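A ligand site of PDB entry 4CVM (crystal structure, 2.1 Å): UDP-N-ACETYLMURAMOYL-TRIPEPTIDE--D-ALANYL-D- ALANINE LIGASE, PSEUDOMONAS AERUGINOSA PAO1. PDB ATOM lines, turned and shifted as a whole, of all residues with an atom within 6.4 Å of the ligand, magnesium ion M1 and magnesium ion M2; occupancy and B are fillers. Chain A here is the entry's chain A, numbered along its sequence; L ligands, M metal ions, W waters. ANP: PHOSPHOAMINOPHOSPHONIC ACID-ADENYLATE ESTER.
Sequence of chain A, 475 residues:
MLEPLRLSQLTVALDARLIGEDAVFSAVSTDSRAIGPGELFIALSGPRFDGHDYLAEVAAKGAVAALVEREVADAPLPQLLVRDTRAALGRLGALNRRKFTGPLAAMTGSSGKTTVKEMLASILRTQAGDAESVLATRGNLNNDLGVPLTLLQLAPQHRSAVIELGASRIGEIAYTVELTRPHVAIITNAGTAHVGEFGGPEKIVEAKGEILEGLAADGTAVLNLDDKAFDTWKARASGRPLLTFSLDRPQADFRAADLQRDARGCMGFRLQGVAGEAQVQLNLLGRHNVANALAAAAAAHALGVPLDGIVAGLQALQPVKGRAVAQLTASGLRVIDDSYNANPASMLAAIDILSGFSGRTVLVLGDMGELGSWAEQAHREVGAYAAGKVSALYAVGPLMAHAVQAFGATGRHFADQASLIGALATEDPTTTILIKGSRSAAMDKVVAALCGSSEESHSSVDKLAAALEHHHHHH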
ATOM      1  N   GLY A 109     -29.245 -18.154 -22.111  1.00  0.00           N
ATOM      2  CA  GLY A 109     -27.957 -18.118 -22.760  1.00  0.00           C
ATOM      3  C   GLY A 109     -28.132 -18.357 -24.246  1.00  0.00           C
ATOM      4  O   GLY A 109     -29.214 -18.675 -24.738  1.00  0.00           O
ATOM      5  N   SER A 110     -27.061 -18.190 -24.986  1.00  0.00           N
ATOM      6  CA  SER A 110     -27.115 -18.460 -26.420  1.00  0.00           C
ATOM      7  C   SER A 110     -26.997 -19.949 -26.637  1.00  0.00           C
ATOM      8  O   SER A 110     -27.655 -20.488 -27.516  1.00  0.00           O
ATOM      9  CB  SER A 110     -26.010 -17.721 -27.187  1.00  0.00           C
ATOM     10  OG  SER A 110     -26.225 -16.342 -27.167  1.00  0.00           O
ATOM     11  N   SER A 111     -26.118 -20.605 -25.872  1.00  0.00           N
ATOM     12  CA  SER A 111     -25.985 -22.026 -26.010  1.00  0.00           C
ATOM     13  C   SER A 111     -25.741 -22.638 -24.634  1.00  0.00           C
ATOM     14  O   SER A 111     -25.268 -21.956 -23.703  1.00  0.00           O
ATOM     15  CB  SER A 111     -24.795 -22.341 -26.962  1.00  0.00           C
ATOM     16  OG  SER A 111     -23.627 -21.834 -26.340  1.00  0.00           O
ATOM     17  N   GLY A 112     -26.105 -23.911 -24.505  1.00  0.00           N
ATOM     18  CA  GLY A 112     -25.903 -24.671 -23.284  1.00  0.00           C
ATOM     19  C   GLY A 112     -27.081 -24.651 -22.314  1.00  0.00           C
ATOM     20  O   GLY A 112     -26.976 -25.263 -21.258  1.00  0.00           O
ATOM     21  N   LYS A 113     -28.188 -24.016 -22.690  1.00  0.00           N
ATOM     22  CA  LYS A 113     -29.389 -23.943 -21.849  1.00  0.00           C
ATOM     23  C   LYS A 113     -29.938 -25.304 -21.492  1.00  0.00           C
ATOM     24  O   LYS A 113     -30.064 -25.638 -20.314  1.00  0.00           O
ATOM     25  CB  LYS A 113     -30.494 -23.133 -22.541  1.00  0.00           C
ATOM     26  CG  LYS A 113     -30.194 -21.660 -22.724  1.00  0.00           C
ATOM     27  CD  LYS A 113     -31.392 -20.919 -23.293  1.00  0.00           C
ATOM     28  CE  LYS A 113     -31.845 -21.384 -24.690  1.00  0.00           C
ATOM     29  NZ  LYS A 113     -30.675 -21.200 -25.616  1.00  0.00           N
ATOM     30  N   THR A 114     -30.183 -26.131 -22.520  1.00  0.00           N
ATOM     31  CA  THR A 114     -30.743 -27.458 -22.322  1.00  0.00           C
ATOM     32  C   THR A 114     -29.796 -28.323 -21.525  1.00  0.00           C
ATOM     33  O   THR A 114     -30.208 -29.082 -20.638  1.00  0.00           O
ATOM     34  CB  THR A 114     -31.194 -28.055 -23.674  1.00  0.00           C
ATOM     35  OG1 THR A 114     -32.330 -27.326 -24.095  1.00  0.00           O
ATOM     36  CG2 THR A 114     -31.671 -29.550 -23.551  1.00  0.00           C
ATOM     37  N   THR A 115     -28.517 -28.219 -21.845  1.00  0.00           N
ATOM     38  CA  THR A 115     -27.547 -29.061 -21.162  1.00  0.00           C
ATOM     39  C   THR A 115     -27.396 -28.695 -19.689  1.00  0.00           C
ATOM     40  O   THR A 115     -27.357 -29.576 -18.832  1.00  0.00           O
ATOM     41  CB  THR A 115     -26.205 -29.005 -21.894  1.00  0.00           C
ATOM     42  OG1 THR A 115     -26.442 -29.347 -23.253  1.00  0.00           O
ATOM     43  CG2 THR A 115     -25.174 -29.959 -21.294  1.00  0.00           C
ATOM     44  N   VAL A 116     -27.298 -27.400 -19.389  1.00  0.00           N
ATOM     45  CA  VAL A 116     -27.245 -26.967 -17.995  1.00  0.00           C
ATOM     46  C   VAL A 116     -28.530 -27.400 -17.261  1.00  0.00           C
ATOM     47  O   VAL A 116     -28.498 -27.904 -16.121  1.00  0.00           O
ATOM     48  CB  VAL A 116     -27.033 -25.466 -17.883  1.00  0.00           C
ATOM     49  CG1 VAL A 116     -27.225 -25.007 -16.468  1.00  0.00           C
ATOM     50  CG2 VAL A 116     -25.639 -25.143 -18.341  1.00  0.00           C
ATOM     51  N   GLY A 139     -38.073 -31.083 -23.432  1.00  0.00           N
ATOM     52  CA  GLY A 139     -37.409 -30.698 -24.705  1.00  0.00           C
ATOM     53  C   GLY A 139     -36.884 -29.289 -24.650  1.00  0.00           C
ATOM     54  O   GLY A 139     -36.124 -28.859 -23.717  1.00  0.00           O
ATOM     55  N   ASN A 140     -37.356 -28.513 -25.614  1.00  0.00           N
ATOM     56  CA  ASN A 140     -36.982 -27.165 -25.714  1.00  0.00           C
ATOM     57  C   ASN A 140     -38.131 -26.176 -25.568  1.00  0.00           C
ATOM     58  O   ASN A 140     -38.116 -25.102 -26.195  1.00  0.00           O
ATOM     59  CB  ASN A 140     -36.321 -27.009 -27.042  1.00  0.00           C
ATOM     60  CG  ASN A 140     -35.124 -26.162 -26.961  1.00  0.00           C
ATOM     61  OD1 ASN A 140     -34.272 -26.368 -26.072  1.00  0.00           O
ATOM     62  ND2 ASN A 140     -35.041 -25.203 -27.860  1.00  0.00           N
ATOM     63  N   ASN A 142     -39.346 -23.445 -24.353  1.00  0.00           N
ATOM     64  CA  ASN A 142     -38.707 -22.360 -23.611  1.00  0.00           C
ATOM     65  C   ASN A 142     -39.079 -20.938 -24.005  1.00  0.00           C
ATOM     66  O   ASN A 142     -38.456 -19.987 -23.496  1.00  0.00           O
ATOM     67  CB  ASN A 142     -37.177 -22.528 -23.655  1.00  0.00           C
ATOM     68  CG  ASN A 142     -36.574 -22.263 -25.031  1.00  0.00           C
ATOM     69  OD1 ASN A 142     -37.205 -21.695 -25.886  1.00  0.00           O
ATOM     70  ND2 ASN A 142     -35.327 -22.634 -25.203  1.00  0.00           N
ATOM     71  N   GLU A 164     -36.028 -23.798 -18.297  1.00  0.00           N
ATOM     72  CA  GLU A 164     -35.277 -23.182 -19.387  1.00  0.00           C
ATOM     73  C   GLU A 164     -36.006 -21.941 -19.955  1.00  0.00           C
ATOM     74  O   GLU A 164     -37.196 -21.982 -20.268  1.00  0.00           O
ATOM     75  CB  GLU A 164     -35.029 -24.265 -20.457  1.00  0.00           C
ATOM     76  CG  GLU A 164     -34.072 -23.877 -21.510  1.00  0.00           C
ATOM     77  CD  GLU A 164     -33.832 -24.971 -22.563  1.00  0.00           C
ATOM     78  OE1 GLU A 164     -33.900 -26.222 -22.295  1.00  0.00           O
ATOM     79  OE2 GLU A 164     -33.485 -24.531 -23.653  1.00  0.00           O
ATOM     80  N   GLY A 166     -35.760 -19.284 -23.102  1.00  0.00           N
ATOM     81  CA  GLY A 166     -35.183 -18.919 -24.387  1.00  0.00           C
ATOM     82  C   GLY A 166     -35.229 -17.425 -24.579  1.00  0.00           C
ATOM     83  O   GLY A 166     -36.187 -16.763 -24.142  1.00  0.00           O
ATOM     84  N   THR A 188     -25.579 -18.726 -19.303  1.00  0.00           N
ATOM     85  CA  THR A 188     -24.396 -19.510 -19.751  1.00  0.00           C
ATOM     86  C   THR A 188     -23.384 -18.679 -20.507  1.00  0.00           C
ATOM     87  O   THR A 188     -22.176 -18.770 -20.260  1.00  0.00           O
ATOM     88  CB  THR A 188     -24.807 -20.691 -20.643  1.00  0.00           C
ATOM     89  OG1 THR A 188     -25.577 -20.194 -21.756  1.00  0.00           O
ATOM     90  CG2 THR A 188     -25.629 -21.679 -19.780  1.00  0.00           C
ATOM     91  N   ASN A 189     -23.906 -17.873 -21.428  1.00  0.00           N
ATOM     92  CA  ASN A 189     -23.110 -17.109 -22.385  1.00  0.00           C
ATOM     93  C   ASN A 189     -24.011 -16.246 -23.284  1.00  0.00           C
ATOM     94  O   ASN A 189     -25.245 -16.412 -23.328  1.00  0.00           O
ATOM     95  CB  ASN A 189     -22.291 -18.033 -23.297  1.00  0.00           C
ATOM     96  CG  ASN A 189     -23.119 -19.128 -23.924  1.00  0.00           C
ATOM     97  OD1 ASN A 189     -24.152 -18.885 -24.567  1.00  0.00           O
ATOM     98  ND2 ASN A 189     -22.706 -20.341 -23.718  1.00  0.00           N
ATOM     99  N   THR A 192     -22.399 -17.277 -28.909  1.00  0.00           N
ATOM    100  CA  THR A 192     -21.587 -18.436 -29.385  1.00  0.00           C
ATOM    101  C   THR A 192     -21.830 -18.794 -30.907  1.00  0.00           C
ATOM    102  O   THR A 192     -22.811 -18.384 -31.507  1.00  0.00           O
ATOM    103  CB  THR A 192     -21.825 -19.678 -28.481  1.00  0.00           C
ATOM    104  OG1 THR A 192     -23.222 -19.846 -28.343  1.00  0.00           O
ATOM    105  CG2 THR A 192     -21.246 -19.460 -27.067  1.00  0.00           C
ATOM    106  N   ALA A 193     -20.905 -19.521 -31.543  1.00  0.00           N
ATOM    107  CA  ALA A 193     -20.999 -19.802 -33.004  1.00  0.00           C
ATOM    108  C   ALA A 193     -22.224 -20.594 -33.459  1.00  0.00           C
ATOM    109  O   ALA A 193     -22.804 -21.396 -32.690  1.00  0.00           O
ATOM    110  CB  ALA A 193     -19.744 -20.529 -33.470  1.00  0.00           C
ATOM    111  N   VAL A 195     -25.266 -20.000 -33.810  1.00  0.00           N
ATOM    112  CA  VAL A 195     -26.555 -19.911 -33.098  1.00  0.00           C
ATOM    113  C   VAL A 195     -27.646 -19.140 -33.869  1.00  0.00           C
ATOM    114  O   VAL A 195     -27.359 -18.169 -34.583  1.00  0.00           O
ATOM    115  CB  VAL A 195     -26.366 -19.403 -31.641  1.00  0.00           C
ATOM    116  CG1 VAL A 195     -27.673 -18.849 -31.075  1.00  0.00           C
ATOM    117  CG2 VAL A 195     -25.904 -20.564 -30.756  1.00  0.00           C
ATOM    118  N   HIS A 288     -16.779 -27.098 -23.905  1.00  0.00           N
ATOM    119  CA  HIS A 288     -17.930 -26.277 -23.516  1.00  0.00           C
ATOM    120  C   HIS A 288     -18.807 -26.975 -22.448  1.00  0.00           C
ATOM    121  O   HIS A 288     -19.520 -26.308 -21.703  1.00  0.00           O
ATOM    122  CB  HIS A 288     -18.780 -25.926 -24.748  1.00  0.00           C
ATOM    123  CG  HIS A 288     -19.337 -27.105 -25.484  1.00  0.00           C
ATOM    124  ND1 HIS A 288     -18.608 -27.814 -26.416  1.00  0.00           N
ATOM    125  CD2 HIS A 288     -20.541 -27.723 -25.407  1.00  0.00           C
ATOM    126  CE1 HIS A 288     -19.343 -28.801 -26.896  1.00  0.00           C
ATOM    127  NE2 HIS A 288     -20.513 -28.780 -26.294  1.00  0.00           N
ATOM    128  N   ASN A 289     -18.787 -28.304 -22.385  1.00  0.00           N
ATOM    129  CA  ASN A 289     -19.636 -29.020 -21.458  1.00  0.00           C
ATOM    130  C   ASN A 289     -19.035 -28.981 -20.028  1.00  0.00           C
ATOM    131  O   ASN A 289     -19.781 -29.106 -19.054  1.00  0.00           O
ATOM    132  CB  ASN A 289     -19.920 -30.425 -21.932  1.00  0.00           C
ATOM    133  CG  ASN A 289     -21.104 -30.482 -22.857  1.00  0.00           C
ATOM    134  OD1 ASN A 289     -22.082 -29.749 -22.666  1.00  0.00           O
ATOM    135  ND2 ASN A 289     -21.025 -31.316 -23.900  1.00  0.00           N
ATOM    136  N   ALA A 291     -17.706 -26.080 -18.901  1.00  0.00           N
ATOM    137  CA  ALA A 291     -18.315 -24.792 -18.479  1.00  0.00           C
ATOM    138  C   ALA A 291     -19.822 -25.008 -18.059  1.00  0.00           C
ATOM    139  O   ALA A 291     -20.248 -24.453 -17.077  1.00  0.00           O
ATOM    140  CB  ALA A 291     -18.207 -23.761 -19.582  1.00  0.00           C
ATOM    141  N   ASN A 292     -20.569 -25.801 -18.823  1.00  0.00           N
ATOM    142  CA  ASN A 292     -21.933 -26.141 -18.492  1.00  0.00           C
ATOM    143  C   ASN A 292     -22.014 -26.849 -17.115  1.00  0.00           C
ATOM    144  O   ASN A 292     -22.867 -26.511 -16.299  1.00  0.00           O
ATOM    145  CB  ASN A 292     -22.635 -26.984 -19.572  1.00  0.00           C
ATOM    146  CG  ASN A 292     -22.806 -26.209 -20.879  1.00  0.00           C
ATOM    147  OD1 ASN A 292     -22.849 -24.976 -20.873  1.00  0.00           O
ATOM    148  ND2 ASN A 292     -23.006 -26.924 -21.958  1.00  0.00           N
ATOM    149  N   ALA A 324     -24.654 -36.977 -30.087  1.00  0.00           N
ATOM    150  CA  ALA A 324     -23.252 -36.988 -29.701  1.00  0.00           C
ATOM    151  C   ALA A 324     -22.974 -38.021 -28.596  1.00  0.00           C
ATOM    152  O   ALA A 324     -22.409 -37.674 -27.586  1.00  0.00           O
ATOM    153  CB  ALA A 324     -22.813 -35.599 -29.283  1.00  0.00           C
ATOM    154  N   ALA A 349     -21.857 -27.529 -35.694  1.00  0.00           N
ATOM    155  CA  ALA A 349     -21.497 -27.836 -34.311  1.00  0.00           C
ATOM    156  C   ALA A 349     -20.816 -29.215 -34.213  1.00  0.00           C
ATOM    157  O   ALA A 349     -19.870 -29.382 -33.438  1.00  0.00           O
ATOM    158  CB  ALA A 349     -22.707 -27.753 -33.389  1.00  0.00           C
ATOM    159  N   ALA A 350     -21.290 -30.191 -35.001  1.00  0.00           N
ATOM    160  CA  ALA A 350     -20.700 -31.544 -35.033  1.00  0.00           C
ATOM    161  C   ALA A 350     -19.254 -31.528 -35.507  1.00  0.00           C
ATOM    162  O   ALA A 350     -18.369 -32.052 -34.853  1.00  0.00           O
ATOM    163  CB  ALA A 350     -21.530 -32.494 -35.945  1.00  0.00           C
ATOM    164  N   ILE A 353     -16.879 -30.249 -32.877  1.00  0.00           N
ATOM    165  CA  ILE A 353     -16.581 -31.292 -31.905  1.00  0.00           C
ATOM    166  C   ILE A 353     -15.518 -32.271 -32.433  1.00  0.00           C
ATOM    167  O   ILE A 353     -14.590 -32.649 -31.696  1.00  0.00           O
ATOM    168  CB  ILE A 353     -17.855 -32.079 -31.450  1.00  0.00           C
ATOM    169  CG1 ILE A 353     -18.791 -31.165 -30.653  1.00  0.00           C
ATOM    170  CG2 ILE A 353     -17.480 -33.293 -30.617  1.00  0.00           C
ATOM    171  CD1 ILE A 353     -20.018 -31.878 -30.097  1.00  0.00           C
HETATM  172  PG  ANP L   1     -31.550 -23.723 -27.999  1.00  0.00           P
HETATM  173  O1G ANP L   1     -31.421 -22.214 -28.001  1.00  0.00           O
HETATM  174  O2G ANP L   1     -32.600 -24.031 -26.949  1.00  0.00           O
HETATM  175  O3G ANP L   1     -31.589 -24.488 -29.255  1.00  0.00           O
HETATM  176  PB  ANP L   1     -29.456 -24.553 -26.001  1.00  0.00           P
HETATM  177  O1B ANP L   1     -28.964 -23.270 -25.405  1.00  0.00           O
HETATM  178  O2B ANP L   1     -30.569 -25.326 -25.281  1.00  0.00           O
HETATM  179  N3B ANP L   1     -29.948 -24.273 -27.632  1.00  0.00           N
HETATM  180  PA  ANP L   1     -27.947 -27.063 -25.895  1.00  0.00           P
HETATM  181  O1A ANP L   1     -27.493 -27.357 -24.472  1.00  0.00           O
HETATM  182  O2A ANP L   1     -29.146 -27.813 -26.508  1.00  0.00           O
HETATM  183  O3A ANP L   1     -28.100 -25.462 -26.133  1.00  0.00           O
HETATM  184  O5' ANP L   1     -26.672 -27.449 -26.799  1.00  0.00           O
HETATM  185  C5' ANP L   1     -26.718 -27.204 -28.235  1.00  0.00           C
HETATM  186  C4' ANP L   1     -25.321 -27.111 -28.829  1.00  0.00           C
HETATM  187  O4' ANP L   1     -24.676 -25.882 -28.487  1.00  0.00           O
HETATM  188  C3' ANP L   1     -24.378 -28.222 -28.330  1.00  0.00           C
HETATM  189  O3' ANP L   1     -24.493 -29.480 -29.012  1.00  0.00           O
HETATM  190  C2' ANP L   1     -23.054 -27.569 -28.540  1.00  0.00           C
HETATM  191  O2' ANP L   1     -22.697 -27.660 -29.932  1.00  0.00           O
HETATM  192  C1' ANP L   1     -23.284 -26.093 -28.229  1.00  0.00           C
HETATM  193  N9  ANP L   1     -23.030 -25.715 -26.818  1.00  0.00           N
HETATM  194  C8  ANP L   1     -23.680 -26.215 -25.720  1.00  0.00           C
HETATM  195  N7  ANP L   1     -23.220 -25.592 -24.587  1.00  0.00           N
HETATM  196  C5  ANP L   1     -22.323 -24.654 -24.984  1.00  0.00           C
HETATM  197  C6  ANP L   1     -21.448 -23.671 -24.328  1.00  0.00           C
HETATM  198  N6  ANP L   1     -21.496 -23.550 -22.981  1.00  0.00           N
HETATM  199  N1  ANP L   1     -20.613 -22.923 -25.104  1.00  0.00           N
HETATM  200  C2  ANP L   1     -20.576 -23.025 -26.444  1.00  0.00           C
HETATM  201  N3  ANP L   1     -21.317 -23.936 -27.086  1.00  0.00           N
HETATM  202  C4  ANP L   1     -22.195 -24.739 -26.443  1.00  0.00           C
HETATM  203 MG    MG M   1     -31.804 -27.074 -26.731  1.00  0.00          MG
HETATM  204 MG    MG M   2     -32.611 -25.626 -25.564  1.00  0.00          MG
HETATM  205  O   HOH W   1     -27.874 -22.923 -28.958  1.00  0.00           O
HETATM  206  O   HOH W   2     -20.583 -21.184 -21.365  1.00  0.00           O
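Of the 26 residues printed, 2 come within 4 Å of magnesium ion M1.
Water W1 bridges N3B of the ligand and O of Ser 110.
Water W2 lies within hydrogen-bond range of N6 of the ligand (3.0 Å), O of Thr 188 (3.1 Å) and ND2 of Asn 189 (3.3 Å).
Of the 26 residues printed, 3 come within 4 Å of magnesium ion M2.
Ser 110 touches the ligand.
Asn 142 touches the ligand.
Asn 189 touches the ligand.
Thr 192 touches the ligand (CG2 to C2, 3.7 Å).
His 288 touches the ligand (CD2 to N9, 3.5 Å).
CB of Ala 349 touches O2' of the ligand, at 3.5 Å.
Hydrophobic or aromatic side chains within 4 Å of the ligand: His 288 and Ala 349.
Within 4 Å of the ligand: Ser 110, Ser 111, Gly 112, Lys 113, Thr 114, Thr 115, Asn 140, Asn 142, Glu 164, Asn 189, Thr 192, His 288, Asn 292 and Ala 349.
The nearest printed residue that does not touch the ligand is Gly 109 (4.6 Å).
Magnesium ion M1 is bound by O2B of the ligand.
Slightly farther from magnesium ion M1 lies OD1 of Asn 140 (2.7 Å).
Slightly farther from magnesium ion M1 lies OG1 of Thr 114 (2.7 Å).
Slightly farther from magnesium ion M1 lies O2A of the ligand (2.8 Å).
The side-chain amide oxygen (OD1) of Asn 140 binds magnesium ion M2 (1.9 Å).
O2B of the ligand is bound to magnesium ion M2.
An oxygen (O2G) of the ligand binds magnesium ion M2, 2.1 Å away.
Magnesium ion M2 is bound by the side-chain hydroxyl (OG1) of Thr 114 (2.3 Å).
OE2 of Glu 164 is bound to magnesium ion M2 (2.4 Å).
Magnesium ion M2 has five donor atoms within binding distance.
N of Thr 114 sits close to O2B of the ligand, at 2.9 Å.
N of Thr 115 is in hydrogen-bond range of O1A of the ligand.
OG1 of Thr 115 sits at hydrogen-bond distance from O1A of the ligand (2.6 Å).
An oxygen (O1B) of the ligand sits at hydrogen-bond distance from the backbone NH of Lys 113, 2.9 Å away.
The side-chain amino group (NZ) of Lys 113 lies within salt-bridge range of an oxygen (O1B) of the ligand (2.7 Å).
OD1 of Asn 292 is in hydrogen-bond range of N6 of the ligand (2.9 Å).
An oxygen (O3A) of the ligand sits at hydrogen-bond distance from the backbone NH of Gly 112, 3.0 Å away.
The side-chain hydroxyl (OG) of Ser 111 sits at hydrogen-bond distance from a nitrogen (N3) of the ligand (3.2 Å).
The side-chain carboxylate (OE2) of Glu 164 sits close to the side-chain amide nitrogen (ND2) of Asn 142 (3.1 Å).
The side-chain amino group (NZ) of Lys 113 is in hydrogen-bond range of the backbone carbonyl oxygen (O) of Gly 109 (3.0 Å).
The side-chain amide oxygen (OD1) of Asn 289 is in hydrogen-bond range of the side-chain amide nitrogen (ND2) of Asn 292.
N of Ser 111 is in hydrogen-bond range of OD1 of Asn 189 (2.9 Å).
The side-chain hydroxyl (OG1) of Thr 192 lies within hydrogen-bond range of the side-chain hydroxyl (OG) of Ser 111 (2.9 Å).
The backbone carbonyl oxygen (O) of Ser 111 lies within hydrogen-bond range of the side-chain hydroxyl (OG1) of Thr 188 (2.6 Å).
The backbone NH (N) of Ser 110 lies within hydrogen-bond range of the side-chain amide oxygen (OD1) of Asn 189 (3.0 Å).
O of Asn 142 sits at hydrogen-bond distance from N of Gly 166, at 2.8 Å.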
